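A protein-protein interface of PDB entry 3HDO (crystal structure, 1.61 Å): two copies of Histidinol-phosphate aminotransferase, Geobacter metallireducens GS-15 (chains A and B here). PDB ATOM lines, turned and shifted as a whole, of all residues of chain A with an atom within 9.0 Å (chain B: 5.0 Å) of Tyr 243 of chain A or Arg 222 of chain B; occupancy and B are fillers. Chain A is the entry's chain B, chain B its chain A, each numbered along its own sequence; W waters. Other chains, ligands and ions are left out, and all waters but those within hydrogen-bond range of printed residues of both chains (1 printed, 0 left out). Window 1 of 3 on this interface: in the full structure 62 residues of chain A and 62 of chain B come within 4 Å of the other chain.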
ATOM      1  N   LEU A  59       4.757 -27.915   7.871  1.00  0.00           N
ATOM      2  CA  LEU A  59       6.192 -27.955   7.609  1.00  0.00           C
ATOM      3  C   LEU A  59       6.582 -27.638   6.168  1.00  0.00           C
ATOM      4  O   LEU A  59       7.761 -27.461   5.870  1.00  0.00           O
ATOM      5  CB  LEU A  59       6.763 -29.315   8.027  1.00  0.00           C
ATOM      6  CG  LEU A  59       6.619 -29.660   9.517  1.00  0.00           C
ATOM      7  CD1 LEU A  59       7.329 -30.974   9.801  1.00  0.00           C
ATOM      8  CD2 LEU A  59       7.204 -28.544  10.378  1.00  0.00           C
ATOM      9  N   ILE A  61       5.729 -24.963   4.730  1.00  0.00           N
ATOM     10  CA  ILE A  61       5.815 -23.503   4.690  1.00  0.00           C
ATOM     11  C   ILE A  61       6.996 -23.007   5.518  1.00  0.00           C
ATOM     12  O   ILE A  61       7.222 -23.481   6.632  1.00  0.00           O
ATOM     13  CB  ILE A  61       4.524 -22.863   5.249  1.00  0.00           C
ATOM     14  CG1 ILE A  61       3.300 -23.464   4.549  1.00  0.00           C
ATOM     15  CG2 ILE A  61       4.567 -21.350   5.073  1.00  0.00           C
ATOM     16  CD1 ILE A  61       3.265 -23.228   3.046  1.00  0.00           C
ATOM     17  N   TYR A  62       7.749 -22.057   4.975  1.00  0.00           N
ATOM     18  CA  TYR A  62       8.900 -21.506   5.688  1.00  0.00           C
ATOM     19  C   TYR A  62       8.508 -20.925   7.032  1.00  0.00           C
ATOM     20  O   TYR A  62       7.420 -20.373   7.185  1.00  0.00           O
ATOM     21  CB  TYR A  62       9.579 -20.424   4.851  1.00  0.00           C
ATOM     22  CG  TYR A  62      10.481 -20.993   3.793  1.00  0.00           C
ATOM     23  CD1 TYR A  62      11.717 -21.536   4.129  1.00  0.00           C
ATOM     24  CD2 TYR A  62      10.081 -21.028   2.458  1.00  0.00           C
ATOM     25  CE1 TYR A  62      12.539 -22.103   3.161  1.00  0.00           C
ATOM     26  CE2 TYR A  62      10.892 -21.591   1.484  1.00  0.00           C
ATOM     27  CZ  TYR A  62      12.118 -22.126   1.842  1.00  0.00           C
ATOM     28  OH  TYR A  62      12.930 -22.676   0.883  1.00  0.00           O
ATOM     29  N   PRO A  63       9.400 -21.035   8.029  1.00  0.00           N
ATOM     30  CA  PRO A  63       9.124 -20.510   9.364  1.00  0.00           C
ATOM     31  C   PRO A  63       9.224 -18.995   9.375  1.00  0.00           C
ATOM     32  O   PRO A  63       9.269 -18.351   8.323  1.00  0.00           O
ATOM     33  CB  PRO A  63      10.210 -21.158  10.211  1.00  0.00           C
ATOM     34  CG  PRO A  63      11.370 -21.157   9.278  1.00  0.00           C
ATOM     35  CD  PRO A  63      10.755 -21.616   7.965  1.00  0.00           C
ATOM     36  N   SER A  64       9.254 -18.434  10.576  1.00  0.00           N
ATOM     37  CA  SER A  64       9.376 -16.997  10.743  1.00  0.00           C
ATOM     38  C   SER A  64      10.853 -16.642  10.639  1.00  0.00           C
ATOM     39  O   SER A  64      11.670 -17.106  11.436  1.00  0.00           O
ATOM     40  CB  SER A  64       8.841 -16.574  12.111  1.00  0.00           C
ATOM     41  OG  SER A  64       9.141 -15.215  12.376  1.00  0.00           O
ATOM     42  N   ALA A  65      11.196 -15.830   9.645  1.00  0.00           N
ATOM     43  CA  ALA A  65      12.579 -15.422   9.460  1.00  0.00           C
ATOM     44  C   ALA A  65      13.030 -14.595  10.659  1.00  0.00           C
ATOM     45  O   ALA A  65      14.142 -14.757  11.157  1.00  0.00           O
ATOM     46  CB  ALA A  65      12.715 -14.607   8.178  1.00  0.00           C
ATOM     47  N   SER A  66      12.143 -13.726  11.128  1.00  0.00           N
ATOM     48  CA  SER A  66      12.442 -12.842  12.253  1.00  0.00           C
ATOM     49  C   SER A  66      12.402 -13.490  13.634  1.00  0.00           C
ATOM     50  O   SER A  66      13.136 -13.075  14.534  1.00  0.00           O
ATOM     51  CB  SER A  66      11.468 -11.663  12.252  1.00  0.00           C
ATOM     52  OG  SER A  66      10.150 -12.098  12.547  1.00  0.00           O
ATOM     53  N   SER A  67      11.548 -14.498  13.801  1.00  0.00           N
ATOM     54  CA  SER A  67      11.388 -15.155  15.098  1.00  0.00           C
ATOM     55  C   SER A  67      10.952 -14.070  16.078  1.00  0.00           C
ATOM     56  O   SER A  67      11.224 -14.142  17.276  1.00  0.00           O
ATOM     57  CB  SER A  67      12.704 -15.783  15.569  1.00  0.00           C
ATOM     58  OG  SER A  67      12.994 -16.969  14.854  1.00  0.00           O
ATOM     59  N   MET A  87      17.350 -14.169  18.032  1.00  0.00           N
ATOM     60  CA  MET A  87      17.276 -15.606  18.240  1.00  0.00           C
ATOM     61  C   MET A  87      18.307 -16.298  17.365  1.00  0.00           C
ATOM     62  O   MET A  87      18.779 -15.731  16.378  1.00  0.00           O
ATOM     63  CB  MET A  87      15.875 -16.127  17.901  1.00  0.00           C
ATOM     64  CG  MET A  87      14.732 -15.365  18.569  1.00  0.00           C
ATOM     65  SD  MET A  87      14.885 -15.254  20.503  1.00  0.00           S
ATOM     66  CE  MET A  87      14.838 -17.140  20.896  1.00  0.00           C
ATOM     67  N   ALA A  88      18.655 -17.527  17.727  1.00  0.00           N
ATOM     68  CA  ALA A  88      19.645 -18.279  16.966  1.00  0.00           C
ATOM     69  C   ALA A  88      19.454 -19.782  17.110  1.00  0.00           C
ATOM     70  O   ALA A  88      18.815 -20.251  18.053  1.00  0.00           O
ATOM     71  CB  ALA A  88      21.044 -17.890  17.420  1.00  0.00           C
ATOM     72  N   ASN A  89      20.009 -20.530  16.158  1.00  0.00           N
ATOM     73  CA  ASN A  89      19.942 -21.990  16.161  1.00  0.00           C
ATOM     74  C   ASN A  89      21.048 -22.470  17.092  1.00  0.00           C
ATOM     75  O   ASN A  89      22.043 -23.044  16.652  1.00  0.00           O
ATOM     76  CB  ASN A  89      20.165 -22.522  14.735  1.00  0.00           C
ATOM     77  CG  ASN A  89      20.178 -24.045  14.661  1.00  0.00           C
ATOM     78  OD1 ASN A  89      19.236 -24.708  15.094  1.00  0.00           O
ATOM     79  ND2 ASN A  89      21.247 -24.604  14.092  1.00  0.00           N
ATOM     80  N   GLU A  93      25.864 -20.280  17.250  1.00  0.00           N
ATOM     81  CA  GLU A  93      25.613 -19.437  16.089  1.00  0.00           C
ATOM     82  C   GLU A  93      25.902 -17.968  16.384  1.00  0.00           C
ATOM     83  O   GLU A  93      26.561 -17.296  15.589  1.00  0.00           O
ATOM     84  CB  GLU A  93      24.163 -19.590  15.609  1.00  0.00           C
ATOM     85  CG  GLU A  93      23.738 -18.518  14.602  1.00  0.00           C
ATOM     86  CD  GLU A  93      22.304 -18.678  14.117  1.00  0.00           C
ATOM     87  OE1 GLU A  93      21.722 -17.677  13.643  1.00  0.00           O
ATOM     88  OE2 GLU A  93      21.764 -19.800  14.195  1.00  0.00           O
ATOM     89  N   ASP A 237      21.672  -9.307  12.853  1.00  0.00           N
ATOM     90  CA  ASP A 237      20.535  -9.690  12.019  1.00  0.00           C
ATOM     91  C   ASP A 237      20.867  -9.696  10.529  1.00  0.00           C
ATOM     92  O   ASP A 237      20.224 -10.401   9.749  1.00  0.00           O
ATOM     93  CB  ASP A 237      19.340  -8.771  12.272  1.00  0.00           C
ATOM     94  CG  ASP A 237      18.349  -9.365  13.253  1.00  0.00           C
ATOM     95  OD1 ASP A 237      17.927 -10.525  13.045  1.00  0.00           O
ATOM     96  OD2 ASP A 237      17.983  -8.674  14.226  1.00  0.00           O
ATOM     97  N   ILE A 239      23.852 -10.562   9.422  1.00  0.00           N
ATOM     98  CA  ILE A 239      24.788 -11.668   9.257  1.00  0.00           C
ATOM     99  C   ILE A 239      24.162 -13.062   9.264  1.00  0.00           C
ATOM    100  O   ILE A 239      24.548 -13.926   8.478  1.00  0.00           O
ATOM    101  CB  ILE A 239      25.877 -11.626  10.360  1.00  0.00           C
ATOM    102  CG1 ILE A 239      26.728 -10.367  10.201  1.00  0.00           C
ATOM    103  CG2 ILE A 239      26.752 -12.879  10.286  1.00  0.00           C
ATOM    104  CD1 ILE A 239      27.722 -10.169  11.319  1.00  0.00           C
ATOM    105  N   ARG A 240      23.205 -13.284  10.156  1.00  0.00           N
ATOM    106  CA  ARG A 240      22.565 -14.591  10.266  1.00  0.00           C
ATOM    107  C   ARG A 240      21.796 -14.981   9.010  1.00  0.00           C
ATOM    108  O   ARG A 240      21.432 -14.129   8.199  1.00  0.00           O
ATOM    109  CB  ARG A 240      21.603 -14.609  11.454  1.00  0.00           C
ATOM    110  CG  ARG A 240      20.367 -13.749  11.253  1.00  0.00           C
ATOM    111  CD  ARG A 240      19.354 -13.975  12.361  1.00  0.00           C
ATOM    112  NE  ARG A 240      18.185 -13.112  12.216  1.00  0.00           N
ATOM    113  CZ  ARG A 240      17.135 -13.380  11.443  1.00  0.00           C
ATOM    114  NH1 ARG A 240      17.092 -14.499  10.732  1.00  0.00           N
ATOM    115  NH2 ARG A 240      16.129 -12.521  11.381  1.00  0.00           N
ATOM    116  N   ASP A 241      21.557 -16.278   8.855  1.00  0.00           N
ATOM    117  CA  ASP A 241      20.799 -16.764   7.711  1.00  0.00           C
ATOM    118  C   ASP A 241      19.382 -16.253   7.923  1.00  0.00           C
ATOM    119  O   ASP A 241      18.891 -16.263   9.053  1.00  0.00           O
ATOM    120  CB  ASP A 241      20.808 -18.292   7.673  1.00  0.00           C
ATOM    121  CG  ASP A 241      19.947 -18.845   6.560  1.00  0.00           C
ATOM    122  OD1 ASP A 241      19.978 -18.269   5.452  1.00  0.00           O
ATOM    123  OD2 ASP A 241      19.246 -19.854   6.786  1.00  0.00           O
ATOM    124  N   HIS A 242      18.720 -15.805   6.859  1.00  0.00           N
ATOM    125  CA  HIS A 242      17.370 -15.282   7.024  1.00  0.00           C
ATOM    126  C   HIS A 242      16.380 -16.280   7.634  1.00  0.00           C
ATOM    127  O   HIS A 242      15.347 -15.880   8.166  1.00  0.00           O
ATOM    128  CB  HIS A 242      16.835 -14.676   5.709  1.00  0.00           C
ATOM    129  CG  HIS A 242      17.108 -15.490   4.482  1.00  0.00           C
ATOM    130  ND1 HIS A 242      16.102 -16.077   3.743  1.00  0.00           N
ATOM    131  CD2 HIS A 242      18.261 -15.759   3.823  1.00  0.00           C
ATOM    132  CE1 HIS A 242      16.622 -16.669   2.683  1.00  0.00           C
ATOM    133  NE2 HIS A 242      17.930 -16.489   2.707  1.00  0.00           N
ATOM    134  N   TYR A 243      16.705 -17.570   7.580  1.00  0.00           N
ATOM    135  CA  TYR A 243      15.864 -18.615   8.177  1.00  0.00           C
ATOM    136  C   TYR A 243      16.769 -19.499   9.045  1.00  0.00           C
ATOM    137  O   TYR A 243      17.351 -20.462   8.548  1.00  0.00           O
ATOM    138  CB  TYR A 243      15.213 -19.494   7.102  1.00  0.00           C
ATOM    139  CG  TYR A 243      14.173 -18.818   6.235  1.00  0.00           C
ATOM    140  CD1 TYR A 243      13.054 -18.205   6.797  1.00  0.00           C
ATOM    141  CD2 TYR A 243      14.295 -18.821   4.847  1.00  0.00           C
ATOM    142  CE1 TYR A 243      12.077 -17.608   5.994  1.00  0.00           C
ATOM    143  CE2 TYR A 243      13.328 -18.231   4.036  1.00  0.00           C
ATOM    144  CZ  TYR A 243      12.222 -17.626   4.616  1.00  0.00           C
ATOM    145  OH  TYR A 243      11.266 -17.039   3.818  1.00  0.00           O
ATOM    146  N   ASN A 244      16.877 -19.190  10.335  1.00  0.00           N
ATOM    147  CA  ASN A 244      17.752 -19.960  11.219  1.00  0.00           C
ATOM    148  C   ASN A 244      17.073 -20.810  12.296  1.00  0.00           C
ATOM    149  O   ASN A 244      17.751 -21.498  13.062  1.00  0.00           O
ATOM    150  CB  ASN A 244      18.771 -19.020  11.874  1.00  0.00           C
ATOM    151  CG  ASN A 244      18.122 -17.999  12.785  1.00  0.00           C
ATOM    152  OD1 ASN A 244      16.990 -17.576  12.555  1.00  0.00           O
ATOM    153  ND2 ASN A 244      18.845 -17.583  13.818  1.00  0.00           N
ATOM    154  N   LEU A 245      15.746 -20.763  12.361  1.00  0.00           N
ATOM    155  CA  LEU A 245      15.002 -21.553  13.343  1.00  0.00           C
ATOM    156  C   LEU A 245      13.757 -22.168  12.723  1.00  0.00           C
ATOM    157  O   LEU A 245      12.872 -21.454  12.252  1.00  0.00           O
ATOM    158  CB  LEU A 245      14.589 -20.700  14.549  1.00  0.00           C
ATOM    159  CG  LEU A 245      15.638 -20.471  15.640  1.00  0.00           C
ATOM    160  CD1 LEU A 245      14.980 -19.811  16.841  1.00  0.00           C
ATOM    161  CD2 LEU A 245      16.252 -21.800  16.060  1.00  0.00           C
ATOM    162  N   ASP A 246      13.687 -23.494  12.738  1.00  0.00           N
ATOM    163  CA  ASP A 246      12.542 -24.188  12.168  1.00  0.00           C
ATOM    164  C   ASP A 246      11.253 -23.924  12.940  1.00  0.00           C
ATOM    165  O   ASP A 246      11.269 -23.388  14.057  1.00  0.00           O
ATOM    166  CB  ASP A 246      12.818 -25.699  12.074  1.00  0.00           C
ATOM    167  CG  ASP A 246      12.924 -26.375  13.431  1.00  0.00           C
ATOM    168  OD1 ASP A 246      11.897 -26.493  14.129  1.00  0.00           O
ATOM    169  OD2 ASP A 246      14.042 -26.799  13.796  1.00  0.00           O
ATOM    170  N   ARG A 247      10.133 -24.303  12.333  1.00  0.00           N
ATOM    171  CA  ARG A 247       8.823 -24.099  12.934  1.00  0.00           C
ATOM    172  C   ARG A 247       8.633 -24.816  14.268  1.00  0.00           C
ATOM    173  O   ARG A 247       8.012 -24.269  15.181  1.00  0.00           O
ATOM    174  CB  ARG A 247       7.728 -24.545  11.963  1.00  0.00           C
ATOM    175  CG  ARG A 247       7.718 -23.786  10.649  1.00  0.00           C
ATOM    176  CD  ARG A 247       6.532 -24.215   9.800  1.00  0.00           C
ATOM    177  NE  ARG A 247       5.282 -23.678  10.321  1.00  0.00           N
ATOM    178  CZ  ARG A 247       4.845 -22.446  10.081  1.00  0.00           C
ATOM    179  NH1 ARG A 247       5.551 -21.623   9.317  1.00  0.00           N
ATOM    180  NH2 ARG A 247       3.707 -22.031  10.616  1.00  0.00           N
ATOM    181  N   LEU A 248       9.158 -26.035  14.383  1.00  0.00           N
ATOM    182  CA  LEU A 248       9.009 -26.780  15.629  1.00  0.00           C
ATOM    183  C   LEU A 248       9.868 -26.168  16.729  1.00  0.00           C
ATOM    184  O   LEU A 248       9.471 -26.152  17.895  1.00  0.00           O
ATOM    185  CB  LEU A 248       9.354 -28.261  15.420  1.00  0.00           C
ATOM    186  CG  LEU A 248       8.489 -28.943  14.350  1.00  0.00           C
ATOM    187  CD1 LEU A 248       8.760 -30.438  14.356  1.00  0.00           C
ATOM    188  CD2 LEU A 248       7.009 -28.685  14.610  1.00  0.00           C
ATOM    189  N   GLN A 250      10.600 -22.994  16.959  1.00  0.00           N
ATOM    190  CA  GLN A 250       9.942 -21.767  17.385  1.00  0.00           C
ATOM    191  C   GLN A 250       8.788 -22.067  18.334  1.00  0.00           C
ATOM    192  O   GLN A 250       8.589 -21.360  19.320  1.00  0.00           O
ATOM    193  CB  GLN A 250       9.445 -20.971  16.180  1.00  0.00           C
ATOM    194  CG  GLN A 250      10.564 -20.280  15.434  1.00  0.00           C
ATOM    195  CD  GLN A 250      10.070 -19.116  14.607  1.00  0.00           C
ATOM    196  OE1 GLN A 250       9.254 -18.316  15.069  1.00  0.00           O
ATOM    197  NE2 GLN A 250      10.573 -19.002  13.386  1.00  0.00           N
ATOM    198  N   ALA B  88      23.416 -30.170   6.561  1.00  0.00           N
ATOM    199  CA  ALA B  88      23.343 -28.797   7.047  1.00  0.00           C
ATOM    200  C   ALA B  88      21.919 -28.390   7.404  1.00  0.00           C
ATOM    201  O   ALA B  88      20.954 -29.032   6.982  1.00  0.00           O
ATOM    202  CB  ALA B  88      23.900 -27.847   5.989  1.00  0.00           C
ATOM    203  N   ASN B  89      21.795 -27.327   8.197  1.00  0.00           N
ATOM    204  CA  ASN B  89      20.489 -26.803   8.582  1.00  0.00           C
ATOM    205  C   ASN B  89      20.086 -25.869   7.449  1.00  0.00           C
ATOM    206  O   ASN B  89      20.140 -24.642   7.581  1.00  0.00           O
ATOM    207  CB  ASN B  89      20.586 -26.035   9.908  1.00  0.00           C
ATOM    208  CG  ASN B  89      19.317 -25.258  10.234  1.00  0.00           C
ATOM    209  OD1 ASN B  89      18.204 -25.777  10.121  1.00  0.00           O
ATOM    210  ND2 ASN B  89      19.484 -24.004  10.651  1.00  0.00           N
ATOM    211  N   GLY B  90      19.695 -26.473   6.330  1.00  0.00           N
ATOM    212  CA  GLY B  90      19.318 -25.714   5.152  1.00  0.00           C
ATOM    213  C   GLY B  90      20.559 -25.557   4.288  1.00  0.00           C
ATOM    214  O   GLY B  90      21.672 -25.568   4.814  1.00  0.00           O
ATOM    215  N   SER B  91      20.397 -25.419   2.975  1.00  0.00           N
ATOM    216  CA  SER B  91      21.574 -25.274   2.126  1.00  0.00           C
ATOM    217  C   SER B  91      22.268 -23.913   2.250  1.00  0.00           C
ATOM    218  O   SER B  91      23.428 -23.778   1.863  1.00  0.00           O
ATOM    219  CB  SER B  91      21.240 -25.585   0.658  1.00  0.00           C
ATOM    220  OG  SER B  91      20.044 -24.959   0.236  1.00  0.00           O
ATOM    221  N   ASP B  92      21.581 -22.908   2.791  1.00  0.00           N
ATOM    222  CA  ASP B  92      22.224 -21.601   2.955  1.00  0.00           C
ATOM    223  C   ASP B  92      23.472 -21.784   3.813  1.00  0.00           C
ATOM    224  O   ASP B  92      24.492 -21.136   3.590  1.00  0.00           O
ATOM    225  CB  ASP B  92      21.292 -20.591   3.635  1.00  0.00           C
ATOM    226  CG  ASP B  92      20.301 -19.964   2.674  1.00  0.00           C
ATOM    227  OD1 ASP B  92      20.461 -20.134   1.449  1.00  0.00           O
ATOM    228  OD2 ASP B  92      19.366 -19.284   3.151  1.00  0.00           O
ATOM    229  N   GLU B  93      23.386 -22.678   4.795  1.00  0.00           N
ATOM    230  CA  GLU B  93      24.521 -22.949   5.673  1.00  0.00           C
ATOM    231  C   GLU B  93      25.743 -23.435   4.897  1.00  0.00           C
ATOM    232  O   GLU B  93      26.862 -22.982   5.148  1.00  0.00           O
ATOM    233  CB  GLU B  93      24.154 -23.993   6.733  1.00  0.00           C
ATOM    234  CG  GLU B  93      25.370 -24.526   7.497  1.00  0.00           C
ATOM    235  CD  GLU B  93      25.026 -25.633   8.480  1.00  0.00           C
ATOM    236  OE1 GLU B  93      25.943 -26.387   8.867  1.00  0.00           O
ATOM    237  OE2 GLU B  93      23.849 -25.739   8.875  1.00  0.00           O
ATOM    238  N   SER B 213      13.778 -28.510   1.422  1.00  0.00           N
ATOM    239  CA  SER B 213      12.783 -27.452   1.556  1.00  0.00           C
ATOM    240  C   SER B 213      11.708 -27.349   0.488  1.00  0.00           C
ATOM    241  O   SER B 213      10.558 -27.038   0.800  1.00  0.00           O
ATOM    242  CB  SER B 213      13.488 -26.104   1.689  1.00  0.00           C
ATOM    243  OG  SER B 213      14.220 -26.062   2.901  1.00  0.00           O
ATOM    244  N   LEU B 218       9.598 -29.654   3.261  1.00  0.00           N
ATOM    245  CA  LEU B 218      10.116 -29.411   4.603  1.00  0.00           C
ATOM    246  C   LEU B 218      10.765 -28.038   4.778  1.00  0.00           C
ATOM    247  O   LEU B 218      11.733 -27.883   5.523  1.00  0.00           O
ATOM    248  CB  LEU B 218      11.100 -30.526   4.981  1.00  0.00           C
ATOM    249  CG  LEU B 218      10.420 -31.877   5.215  1.00  0.00           C
ATOM    250  CD1 LEU B 218      11.466 -32.978   5.377  1.00  0.00           C
ATOM    251  CD2 LEU B 218       9.543 -31.782   6.456  1.00  0.00           C
ATOM    252  N   ALA B 219      10.208 -27.035   4.105  1.00  0.00           N
ATOM    253  CA  ALA B 219      10.738 -25.677   4.194  1.00  0.00           C
ATOM    254  C   ALA B 219      10.698 -25.150   5.628  1.00  0.00           C
ATOM    255  O   ALA B 219      11.473 -24.262   5.991  1.00  0.00           O
ATOM    256  CB  ALA B 219       9.951 -24.750   3.271  1.00  0.00           C
ATOM    257  N   GLY B 220       9.796 -25.700   6.436  1.00  0.00           N
ATOM    258  CA  GLY B 220       9.681 -25.276   7.820  1.00  0.00           C
ATOM    259  C   GLY B 220      10.617 -26.044   8.737  1.00  0.00           C
ATOM    260  O   GLY B 220      10.632 -25.825   9.945  1.00  0.00           O
ATOM    261  N   MET B 221      11.398 -26.939   8.138  1.00  0.00           N
ATOM    262  CA  MET B 221      12.361 -27.791   8.832  1.00  0.00           C
ATOM    263  C   MET B 221      13.575 -27.825   7.926  1.00  0.00           C
ATOM    264  O   MET B 221      13.844 -28.842   7.283  1.00  0.00           O
ATOM    265  CB  MET B 221      11.814 -29.210   8.936  1.00  0.00           C
ATOM    266  CG  MET B 221      10.540 -29.327   9.707  1.00  0.00           C
ATOM    267  SD  MET B 221      11.024 -29.697  11.493  1.00  0.00           S
ATOM    268  CE  MET B 221      11.729 -31.473  11.175  1.00  0.00           C
ATOM    269  N   ARG B 222      14.309 -26.721   7.878  1.00  0.00           N
ATOM    270  CA  ARG B 222      15.460 -26.629   6.996  1.00  0.00           C
ATOM    271  C   ARG B 222      16.545 -27.687   7.168  1.00  0.00           C
ATOM    272  O   ARG B 222      17.266 -27.747   8.166  1.00  0.00           O
ATOM    273  CB  ARG B 222      16.036 -25.215   7.062  1.00  0.00           C
ATOM    274  CG  ARG B 222      15.022 -24.184   6.569  1.00  0.00           C
ATOM    275  CD  ARG B 222      15.507 -22.747   6.684  1.00  0.00           C
ATOM    276  NE  ARG B 222      16.630 -22.451   5.802  1.00  0.00           N
ATOM    277  CZ  ARG B 222      17.901 -22.427   6.193  1.00  0.00           C
ATOM    278  NH1 ARG B 222      18.212 -22.681   7.456  1.00  0.00           N
ATOM    279  NH2 ARG B 222      18.859 -22.145   5.322  1.00  0.00           N
ATOM    280  N   ILE B 223      16.626 -28.531   6.149  1.00  0.00           N
ATOM    281  CA  ILE B 223      17.582 -29.623   6.085  1.00  0.00           C
ATOM    282  C   ILE B 223      18.169 -29.572   4.686  1.00  0.00           C
ATOM    283  O   ILE B 223      17.433 -29.579   3.701  1.00  0.00           O
ATOM    284  CB  ILE B 223      16.875 -30.981   6.278  1.00  0.00           C
ATOM    285  CG1 ILE B 223      16.177 -31.015   7.636  1.00  0.00           C
ATOM    286  CG2 ILE B 223      17.878 -32.120   6.150  1.00  0.00           C
ATOM    287  CD1 ILE B 223      15.149 -32.133   7.765  1.00  0.00           C
ATOM    288  N   GLY B 224      19.493 -29.496   4.597  1.00  0.00           N
ATOM    289  CA  GLY B 224      20.138 -29.453   3.299  1.00  0.00           C
ATOM    290  C   GLY B 224      21.398 -30.288   3.334  1.00  0.00           C
ATOM    291  O   GLY B 224      21.748 -30.852   4.368  1.00  0.00           O
ATOM    292  N   LEU B 245      22.048 -29.788  13.264  1.00  0.00           N
ATOM    293  CA  LEU B 245      20.725 -30.331  12.962  1.00  0.00           C
ATOM    294  C   LEU B 245      20.115 -30.929  14.220  1.00  0.00           C
ATOM    295  O   LEU B 245      20.731 -31.765  14.878  1.00  0.00           O
ATOM    296  CB  LEU B 245      20.799 -31.409  11.875  1.00  0.00           C
ATOM    297  CG  LEU B 245      20.861 -30.953  10.415  1.00  0.00           C
ATOM    298  CD1 LEU B 245      20.857 -32.178   9.516  1.00  0.00           C
ATOM    299  CD2 LEU B 245      19.671 -30.057  10.089  1.00  0.00           C
HETATM  300  O   HOH W   1      14.188 -24.769   9.802  1.00  0.00           O
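Asn 89 of chain B touches its own counterpart, Asn 89 of chain A. 4 positions are printed for both chains. Of the 20 pairs that touch across the chains among the printed residues, 1 has its exchanged pair printed and touching as well.
Water W1 bridges N of Arg 222 of chain B (2.7 Å) and N of Asp 246 of chain A (3.2 Å).
Of the printed residues of chain B, Ile 61 of chain A touches Ala 219 (3.98 Å) and Gly 220 (3.3 Å). Printed residues of chain B within 4 Å of His 242 of chain A: Asp 92 (3.2 Å). Tyr 243 of chain A touches just one residue of chain B: Arg 222. Of the printed residues of chain A, Ser 213 of chain B touches Tyr 62. Gly 220 of chain B touches just these residues of chain A: Leu 59 (2.8 Å), Ile 61 (3.3 Å), Pro 63 (3.8 Å), Asp 246 (3.1 Å) and Arg 247 (2.9 Å). Of chain A, only Asp 241 (2.7 Å) and Tyr 243 (2.6 Å) come within 4 Å of Arg 222 of chain B. No residue of chain A comes within 4 Å of Ile 223 of chain B.
The side-chain carboxylate of Glu 93 of chain A sits at hydrogen-bond distance from the side-chain amide nitrogen of Asn 244 of chain A (2.9 Å). The backbone carbonyl oxygen (O) of Arg 222 of chain B lies within hydrogen-bond range of the backbone NH (N) of Gly 90 of chain B, 3.3 Å away.
The backbone carbonyl oxygen (O) of Leu 59 of chain A is in hydrogen-bond range of the backbone NH (N) of Gly 220 of chain B (2.8 Å). The backbone NH (N) of Arg 247 of chain A sits at hydrogen-bond distance from the backbone carbonyl oxygen (O) of Gly 220 of chain B (2.9 Å). NH1 of Arg 222 of chain B sits at hydrogen-bond distance from O of Tyr 243 of chain A, at 2.6 Å. The backbone carbonyl oxygen of Leu 59 of chain A lies within hydrogen-bond range of the backbone NH of Ala 219 of chain B (3.0 Å). OD2 of Asp 92 of chain B sits at hydrogen-bond distance from NE2 of His 242 of chain A (3.2 Å). The backbone carbonyl oxygen (O) of Ile 61 of chain A lies close to the backbone NH (N) of Gly 220 of chain B (3.4 Å). The guanidinium group of Arg 222 of chain B is in salt-bridge range of the side-chain carboxylate of Asp 241 of chain A, 2.7 Å away. The side-chain carboxylate (OD2) of Asp 92 of chain B lies close to the side-chain carboxylate (OD1) of Asp 241 of chain A, 2.6 Å away.
Hydrophobic or aromatic side chains of chain A within 4 Å of the printed part of chain B: Leu 59, Tyr 62, Pro 63, His 242, Tyr 243 and Leu 248. Of the 15 printed residues of chain B, 8 touch a printed residue of chain A. Printed residues of chain B that touch a printed residue of chain A: Asn 89, Asp 92, Ser 213, Leu 218, Ala 219, Gly 220, Met 221 and Arg 222. Hydrophobic or aromatic side chains of chain B within 4 Å of the printed part of chain A: Ala 219 and Met 221. Among the printed residues, 20 pairs touch across the chains. Among the printed residues, Asp or Glu carboxylates within 4 Å of a Lys or Arg side-chain nitrogen of the other chain: Asp 241 of chain A with Arg 222 of chain B (2.7 Å).
Among the printed residues, merely in contact across the chains: Leu 59 of chain A with Leu 218 of chain B (3.2 Å), Leu 59 of chain A with Met 221 of chain B (3.5 Å), Ile 61 of chain A with Ala 219 of chain B (3.98 Å), Tyr 62 of chain A with Ser 213 of chain B (3.6 Å), Tyr 62 of chain A with Ala 219 of chain B (3.3 Å), Pro 63 of chain A with Ala 219 of chain B (3.4 Å), Pro 63 of chain A with Gly 220 of chain B (3.8 Å), Asn 89 of chain A with Asn 89 of chain B (3.9 Å), Asn 244 of chain A with Asn 89 of chain B (3.9 Å), Asp 246 of chain A with Gly 220 of chain B (3.1 Å), Asp 246 of chain A with Met 221 of chain B (3.9 Å) and Leu 248 of chain A with Met 221 of chain B (3.7 Å).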
